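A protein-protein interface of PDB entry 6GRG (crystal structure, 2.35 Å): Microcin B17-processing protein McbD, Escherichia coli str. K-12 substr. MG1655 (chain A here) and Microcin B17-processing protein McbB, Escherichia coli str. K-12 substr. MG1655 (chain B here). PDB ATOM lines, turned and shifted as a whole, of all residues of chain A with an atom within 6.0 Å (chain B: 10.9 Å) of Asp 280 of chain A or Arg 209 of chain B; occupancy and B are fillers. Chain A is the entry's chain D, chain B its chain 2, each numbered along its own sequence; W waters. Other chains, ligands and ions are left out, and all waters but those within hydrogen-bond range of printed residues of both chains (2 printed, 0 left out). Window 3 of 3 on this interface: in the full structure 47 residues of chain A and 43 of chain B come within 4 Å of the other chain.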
ATOM      1  N   GLU A  36     -13.623   0.776  18.563  1.00  0.00           N
ATOM      2  CA  GLU A  36     -14.878   0.734  19.295  1.00  0.00           C
ATOM      3  C   GLU A  36     -16.036   0.500  18.322  1.00  0.00           C
ATOM      4  O   GLU A  36     -17.169   0.895  18.598  1.00  0.00           O
ATOM      5  CB  GLU A  36     -15.023   2.008  20.107  1.00  0.00           C
ATOM      6  CG  GLU A  36     -13.938   2.138  21.132  1.00  0.00           C
ATOM      7  CD  GLU A  36     -14.085   3.361  22.008  1.00  0.00           C
ATOM      8  OE1 GLU A  36     -14.400   4.443  21.487  1.00  0.00           O
ATOM      9  OE2 GLU A  36     -13.885   3.220  23.205  1.00  0.00           O
ATOM     10  N   ARG A  37     -15.722  -0.175  17.208  1.00  0.00           N
ATOM     11  CA  ARG A  37     -16.693  -0.662  16.228  1.00  0.00           C
ATOM     12  C   ARG A  37     -17.650  -1.662  16.892  1.00  0.00           C
ATOM     13  O   ARG A  37     -18.869  -1.645  16.633  1.00  0.00           O
ATOM     14  CB  ARG A  37     -15.949  -1.313  15.060  1.00  0.00           C
ATOM     15  CG  ARG A  37     -15.212  -0.316  14.181  1.00  0.00           C
ATOM     16  CD  ARG A  37     -14.099  -1.005  13.412  1.00  0.00           C
ATOM     17  NE  ARG A  37     -13.605  -0.164  12.329  1.00  0.00           N
ATOM     18  CZ  ARG A  37     -12.476  -0.361  11.649  1.00  0.00           C
ATOM     19  NH1 ARG A  37     -11.698  -1.384  11.966  1.00  0.00           N
ATOM     20  NH2 ARG A  37     -12.129   0.479  10.680  1.00  0.00           N
ATOM     21  N   THR A 278      -9.878   3.032  32.718  1.00  0.00           N
ATOM     22  CA  THR A 278     -10.874   3.966  33.243  1.00  0.00           C
ATOM     23  C   THR A 278     -12.304   3.525  32.876  1.00  0.00           C
ATOM     24  O   THR A 278     -12.512   2.744  31.973  1.00  0.00           O
ATOM     25  CB  THR A 278     -10.611   5.344  32.626  1.00  0.00           C
ATOM     26  OG1 THR A 278     -10.725   5.182  31.209  1.00  0.00           O
ATOM     27  CG2 THR A 278      -9.243   5.908  32.951  1.00  0.00           C
ATOM     28  N   ASP A 279     -13.307   4.115  33.532  1.00  0.00           N
ATOM     29  CA  ASP A 279     -14.734   3.898  33.174  1.00  0.00           C
ATOM     30  C   ASP A 279     -15.033   4.330  31.718  1.00  0.00           C
ATOM     31  O   ASP A 279     -15.895   3.731  31.070  1.00  0.00           O
ATOM     32  CB  ASP A 279     -15.668   4.580  34.186  1.00  0.00           C
ATOM     33  CG  ASP A 279     -16.088   3.693  35.352  1.00  0.00           C
ATOM     34  OD1 ASP A 279     -16.403   4.251  36.434  1.00  0.00           O
ATOM     35  OD2 ASP A 279     -16.123   2.446  35.174  1.00  0.00           O
ATOM     36  N   ASP A 280     -14.322   5.343  31.195  1.00  0.00           N
ATOM     37  CA  ASP A 280     -14.524   5.843  29.834  1.00  0.00           C
ATOM     38  C   ASP A 280     -14.146   4.744  28.838  1.00  0.00           C
ATOM     39  O   ASP A 280     -14.510   4.814  27.662  1.00  0.00           O
ATOM     40  CB  ASP A 280     -13.745   7.136  29.563  1.00  0.00           C
ATOM     41  N   ASP A 281     -13.422   3.726  29.320  1.00  0.00           N
ATOM     42  CA  ASP A 281     -13.063   2.568  28.518  1.00  0.00           C
ATOM     43  C   ASP A 281     -14.269   1.633  28.355  1.00  0.00           C
ATOM     44  O   ASP A 281     -14.293   0.844  27.423  1.00  0.00           O
ATOM     45  CB  ASP A 281     -11.865   1.828  29.121  1.00  0.00           C
ATOM     46  CG  ASP A 281     -10.553   2.587  28.973  1.00  0.00           C
ATOM     47  OD1 ASP A 281     -10.130   2.790  27.816  1.00  0.00           O
ATOM     48  OD2 ASP A 281      -9.959   2.971  30.010  1.00  0.00           O
ATOM     49  N   ILE A 282     -15.249   1.708  29.268  1.00  0.00           N
ATOM     50  CA  ILE A 282     -16.445   0.849  29.211  1.00  0.00           C
ATOM     51  C   ILE A 282     -17.527   1.543  28.374  1.00  0.00           C
ATOM     52  O   ILE A 282     -18.020   2.620  28.776  1.00  0.00           O
ATOM     53  CB  ILE A 282     -16.956   0.501  30.623  1.00  0.00           C
ATOM     54  CG1 ILE A 282     -15.857  -0.110  31.499  1.00  0.00           C
ATOM     55  CG2 ILE A 282     -18.176  -0.414  30.528  1.00  0.00           C
ATOM     56  CD1 ILE A 282     -15.310  -1.423  30.952  1.00  0.00           C
ATOM     57  N   ILE A 283     -17.884   0.921  27.234  1.00  0.00           N
ATOM     58  CA  ILE A 283     -18.889   1.431  26.283  1.00  0.00           C
ATOM     59  C   ILE A 283     -20.150   0.550  26.281  1.00  0.00           C
ATOM     60  O   ILE A 283     -21.114   0.881  25.593  1.00  0.00           O
ATOM     61  CB  ILE A 283     -18.317   1.555  24.851  1.00  0.00           C
ATOM     62  CG1 ILE A 283     -18.115   0.196  24.170  1.00  0.00           C
ATOM     63  CG2 ILE A 283     -17.041   2.380  24.845  1.00  0.00           C
ATOM     64  CD1 ILE A 283     -17.556   0.270  22.762  1.00  0.00           C
ATOM     65  N   SER B 202     -20.506   1.062   6.441  1.00  0.00           N
ATOM     66  CA  SER B 202     -21.519   0.587   7.376  1.00  0.00           C
ATOM     67  C   SER B 202     -20.890   0.423   8.770  1.00  0.00           C
ATOM     68  O   SER B 202     -21.431   0.914   9.772  1.00  0.00           O
ATOM     69  CB  SER B 202     -22.174  -0.687   6.893  1.00  0.00           C
ATOM     70  OG  SER B 202     -23.046  -1.219   7.885  1.00  0.00           O
ATOM     71  N   ARG B 203     -19.717  -0.221   8.833  1.00  0.00           N
ATOM     72  CA  ARG B 203     -19.104  -0.531  10.119  1.00  0.00           C
ATOM     73  C   ARG B 203     -18.703   0.769  10.835  1.00  0.00           C
ATOM     74  O   ARG B 203     -18.824   0.840  12.049  1.00  0.00           O
ATOM     75  CB  ARG B 203     -17.962  -1.542   9.953  1.00  0.00           C
ATOM     76  CG  ARG B 203     -17.482  -2.178  11.256  1.00  0.00           C
ATOM     77  CD  ARG B 203     -16.261  -3.091  11.123  1.00  0.00           C
ATOM     78  NE  ARG B 203     -15.152  -2.485  10.381  1.00  0.00           N
ATOM     79  CZ  ARG B 203     -14.115  -3.148   9.861  1.00  0.00           C
ATOM     80  NH1 ARG B 203     -13.895  -4.411  10.186  1.00  0.00           N
ATOM     81  NH2 ARG B 203     -13.296  -2.530   9.028  1.00  0.00           N
ATOM     82  N   GLU B 204     -18.246   1.792  10.093  1.00  0.00           N
ATOM     83  CA  GLU B 204     -17.906   3.092  10.703  1.00  0.00           C
ATOM     84  C   GLU B 204     -19.197   3.777  11.185  1.00  0.00           C
ATOM     85  O   GLU B 204     -19.269   4.228  12.312  1.00  0.00           O
ATOM     86  CB  GLU B 204     -17.167   4.028   9.740  1.00  0.00           C
ATOM     87  CG  GLU B 204     -15.711   3.694   9.470  1.00  0.00           C
ATOM     88  CD  GLU B 204     -14.863   3.272  10.660  1.00  0.00           C
ATOM     89  OE1 GLU B 204     -14.349   4.158  11.423  1.00  0.00           O
ATOM     90  OE2 GLU B 204     -14.695   2.043  10.801  1.00  0.00           O
ATOM     91  N   GLU B 205     -20.209   3.827  10.309  1.00  0.00           N
ATOM     92  CA  GLU B 205     -21.468   4.497  10.568  1.00  0.00           C
ATOM     93  C   GLU B 205     -22.166   3.820  11.755  1.00  0.00           C
ATOM     94  O   GLU B 205     -22.687   4.521  12.630  1.00  0.00           O
ATOM     95  CB  GLU B 205     -22.360   4.508   9.323  1.00  0.00           C
ATOM     96  CG  GLU B 205     -23.463   5.568   9.390  1.00  0.00           C
ATOM     97  CD  GLU B 205     -24.764   5.330   8.618  1.00  0.00           C
ATOM     98  OE1 GLU B 205     -25.153   4.150   8.384  1.00  0.00           O
ATOM     99  OE2 GLU B 205     -25.411   6.343   8.260  1.00  0.00           O
ATOM    100  N   LYS B 206     -22.144   2.478  11.815  1.00  0.00           N
ATOM    101  CA  LYS B 206     -22.885   1.729  12.850  1.00  0.00           C
ATOM    102  C   LYS B 206     -21.984   1.273  14.020  1.00  0.00           C
ATOM    103  O   LYS B 206     -22.395   0.464  14.840  1.00  0.00           O
ATOM    104  CB  LYS B 206     -23.640   0.582  12.185  1.00  0.00           C
ATOM    105  CG  LYS B 206     -24.818   1.063  11.352  1.00  0.00           C
ATOM    106  CD  LYS B 206     -25.434   0.030  10.448  1.00  0.00           C
ATOM    107  CE  LYS B 206     -26.782   0.475   9.929  1.00  0.00           C
ATOM    108  NZ  LYS B 206     -27.406  -0.575   9.095  1.00  0.00           N
ATOM    109  N   SER B 207     -20.820   1.898  14.195  1.00  0.00           N
ATOM    110  CA  SER B 207     -19.951   1.611  15.334  1.00  0.00           C
ATOM    111  C   SER B 207     -20.698   1.792  16.646  1.00  0.00           C
ATOM    112  O   SER B 207     -21.530   2.702  16.793  1.00  0.00           O
ATOM    113  CB  SER B 207     -18.716   2.443  15.332  1.00  0.00           C
ATOM    114  OG  SER B 207     -17.858   1.986  14.312  1.00  0.00           O
ATOM    115  N   PHE B 208     -20.330   0.924  17.595  1.00  0.00           N
ATOM    116  CA  PHE B 208     -20.904   0.883  18.925  1.00  0.00           C
ATOM    117  C   PHE B 208     -20.597   2.201  19.653  1.00  0.00           C
ATOM    118  O   PHE B 208     -21.421   2.693  20.407  1.00  0.00           O
ATOM    119  CB  PHE B 208     -20.401  -0.374  19.638  1.00  0.00           C
ATOM    120  CG  PHE B 208     -21.123  -0.723  20.905  1.00  0.00           C
ATOM    121  CD1 PHE B 208     -22.481  -0.486  21.051  1.00  0.00           C
ATOM    122  CD2 PHE B 208     -20.436  -1.296  21.957  1.00  0.00           C
ATOM    123  CE1 PHE B 208     -23.130  -0.804  22.234  1.00  0.00           C
ATOM    124  CE2 PHE B 208     -21.087  -1.613  23.139  1.00  0.00           C
ATOM    125  CZ  PHE B 208     -22.433  -1.369  23.276  1.00  0.00           C
ATOM    126  N   ARG B 209     -19.399   2.740  19.419  1.00  0.00           N
ATOM    127  CA  ARG B 209     -19.087   4.137  19.649  1.00  0.00           C
ATOM    128  C   ARG B 209     -18.337   4.700  18.435  1.00  0.00           C
ATOM    129  O   ARG B 209     -17.152   4.430  18.270  1.00  0.00           O
ATOM    130  CB  ARG B 209     -18.250   4.321  20.915  1.00  0.00           C
ATOM    131  CG  ARG B 209     -18.049   5.791  21.265  1.00  0.00           C
ATOM    132  CD  ARG B 209     -18.014   6.101  22.749  1.00  0.00           C
ATOM    133  NE  ARG B 209     -16.690   5.814  23.273  1.00  0.00           N
ATOM    134  CZ  ARG B 209     -16.365   5.827  24.555  1.00  0.00           C
ATOM    135  NH1 ARG B 209     -17.234   6.253  25.455  1.00  0.00           N
ATOM    136  NH2 ARG B 209     -15.171   5.406  24.934  1.00  0.00           N
ATOM    137  N   ARG B 210     -19.064   5.420  17.561  1.00  0.00           N
ATOM    138  CA  ARG B 210     -18.502   6.147  16.412  1.00  0.00           C
ATOM    139  C   ARG B 210     -17.240   6.840  16.924  1.00  0.00           C
ATOM    140  O   ARG B 210     -17.235   7.510  17.987  1.00  0.00           O
ATOM    141  CB  ARG B 210     -19.458   7.205  15.815  1.00  0.00           C
ATOM    142  CG  ARG B 210     -20.437   6.730  14.740  1.00  0.00           C
ATOM    143  CD  ARG B 210     -21.465   7.765  14.270  1.00  0.00           C
ATOM    144  N   ASN B 211     -16.153   6.584  16.214  1.00  0.00           N
ATOM    145  CA  ASN B 211     -14.991   7.396  16.306  1.00  0.00           C
ATOM    146  C   ASN B 211     -15.299   8.683  15.536  1.00  0.00           C
ATOM    147  O   ASN B 211     -15.392   8.667  14.307  1.00  0.00           O
ATOM    148  CB  ASN B 211     -13.798   6.605  15.792  1.00  0.00           C
ATOM    149  CG  ASN B 211     -12.640   7.451  15.320  1.00  0.00           C
ATOM    150  OD1 ASN B 211     -12.412   8.564  15.802  1.00  0.00           O
ATOM    151  ND2 ASN B 211     -11.881   6.891  14.397  1.00  0.00           N
ATOM    152  N   GLU B 212     -15.458   9.799  16.253  1.00  0.00           N
ATOM    153  CA  GLU B 212     -15.888  11.042  15.609  1.00  0.00           C
ATOM    154  C   GLU B 212     -14.803  11.571  14.642  1.00  0.00           C
ATOM    155  O   GLU B 212     -15.114  12.393  13.805  1.00  0.00           O
ATOM    156  CB  GLU B 212     -16.389  12.038  16.666  1.00  0.00           C
ATOM    157  CG  GLU B 212     -17.630  11.574  17.467  1.00  0.00           C
ATOM    158  CD  GLU B 212     -18.800  10.862  16.763  1.00  0.00           C
ATOM    159  OE1 GLU B 212     -18.991  11.056  15.539  1.00  0.00           O
ATOM    160  OE2 GLU B 212     -19.554  10.098  17.449  1.00  0.00           O
ATOM    161  N   MET B 213     -13.573  11.025  14.664  1.00  0.00           N
ATOM    162  CA  MET B 213     -12.518  11.351  13.683  1.00  0.00           C
ATOM    163  C   MET B 213     -12.295  10.195  12.690  1.00  0.00           C
ATOM    164  O   MET B 213     -11.186   9.997  12.219  1.00  0.00           O
ATOM    165  CB  MET B 213     -11.198  11.648  14.395  1.00  0.00           C
ATOM    166  CG  MET B 213     -11.266  12.829  15.314  1.00  0.00           C
ATOM    167  SD  MET B 213     -11.391  14.374  14.391  1.00  0.00           S
ATOM    168  CE  MET B 213     -13.147  14.733  14.419  1.00  0.00           C
ATOM    169  N   SER B 214     -13.365   9.479  12.329  1.00  0.00           N
ATOM    170  CA  SER B 214     -13.338   8.399  11.330  1.00  0.00           C
ATOM    171  C   SER B 214     -13.064   8.932   9.923  1.00  0.00           C
ATOM    172  O   SER B 214     -13.584   9.980   9.584  1.00  0.00           O
ATOM    173  CB  SER B 214     -14.645   7.638  11.303  1.00  0.00           C
ATOM    174  OG  SER B 214     -14.688   6.764  10.174  1.00  0.00           O
ATOM    175  N   ASN B 217     -15.994   9.962   7.643  1.00  0.00           N
ATOM    176  CA  ASN B 217     -16.378  11.392   7.611  1.00  0.00           C
ATOM    177  C   ASN B 217     -15.837  12.083   6.347  1.00  0.00           C
ATOM    178  O   ASN B 217     -16.562  12.858   5.693  1.00  0.00           O
ATOM    179  CB  ASN B 217     -15.914  12.175   8.843  1.00  0.00           C
ATOM    180  CG  ASN B 217     -16.580  11.719  10.122  1.00  0.00           C
ATOM    181  OD1 ASN B 217     -17.644  11.103  10.091  1.00  0.00           O
ATOM    182  ND2 ASN B 217     -15.947  11.987  11.252  1.00  0.00           N
HETATM  183  O   HOH W   1     -14.305   3.111  16.743  1.00  0.00           O
HETATM  184  O   HOH W   2     -14.965   0.110   9.025  1.00  0.00           O
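NE of Arg 37 of chain A lies within salt-bridge range of OE2 of Glu 204 of chain B (2.9 Å). The backbone NH (N) of Phe 208 of chain B is in hydrogen-bond range of the backbone carbonyl oxygen (O) of Glu 36 of chain A, 3.3 Å away. The backbone NH (N) of Phe 208 of chain B is in hydrogen-bond range of the backbone carbonyl oxygen (O) of Arg 37 of chain A. OE2 of Glu 36 of chain A lies within salt-bridge range of NH2 of Arg 209 of chain B, at 3.1 Å. The backbone carbonyl oxygen (O) of Asp 280 of chain A is in hydrogen-bond range of the guanidinium group (NH2) of Arg 209 of chain B (2.9 Å). The guanidinium group (NE) of Arg 37 of chain A sits close to the guanidinium group (NE) of Arg 203 of chain B, 3.4 Å away.
Water W2 lies within hydrogen-bond range of the side-chain carboxylate of Glu 204 of chain B (2.6 Å), the guanidinium group of Arg 203 of chain B (2.9 Å) and the guanidinium group of Arg 37 of chain A (3.3 Å). Water W1 bridges the backbone NH of Glu 36 of chain A and the backbone carbonyl oxygen of Arg 209 of chain B.
Arg 209 of chain B touches just these residues of chain A: Glu 36 (3.0 Å), Asp 280 (2.9 Å) and Ile 283 (3.5 Å). Of the printed residues of chain B, Glu 36 of chain A touches Ser 207 (3.9 Å), Phe 208 (3.3 Å) and Arg 209 (3.0 Å). No residue of chain B comes within 4 Å of Thr 278 of chain A. No residue of chain B comes within 4 Å of Ile 282 of chain A. Printed residues of chain A within 4 Å of Arg 203 of chain B: Arg 37. Of the printed residues of chain A, Ser 207 of chain B touches Glu 36 (3.9 Å) and Arg 37 (3.5 Å). The nearest residue of chain B that does not touch Asp 280 of chain A is Phe 208 of chain B (10.2 Å). The nearest residue of chain A that does not touch Arg 209 of chain B is Arg 37 of chain A (4.9 Å).
Among the printed residues, merely in contact across the chains: Glu 36 of chain A with Ser 207 of chain B (3.9 Å), Arg 37 of chain A with Ser 207 of chain B (3.5 Å), Ile 283 of chain A with Phe 208 of chain B (3.4 Å) and Ile 283 of chain A with Arg 209 of chain B (3.5 Å).
O of Arg 203 of chain B sits at hydrogen-bond distance from OG of Ser 207 of chain B (2.7 Å). The side-chain hydroxyl (OG) of Ser 207 of chain B is in hydrogen-bond range of the backbone carbonyl oxygen (O) of Glu 204 of chain B (3.3 Å). OE1 of Glu 204 of chain B sits at hydrogen-bond distance from OG of Ser 214 of chain B (2.9 Å).
Printed residues of chain B that touch a printed residue of chain A: Arg 203, Glu 204, Ser 207, Phe 208 and Arg 209. Among the printed residues, 10 pairs touch across the chains. Among the printed residues, Asp or Glu carboxylates within 4 Å of a Lys or Arg side-chain nitrogen of the other chain: Glu 36 of chain A with Arg 209 of chain B and Arg 37 of chain A with Glu 204 of chain B.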
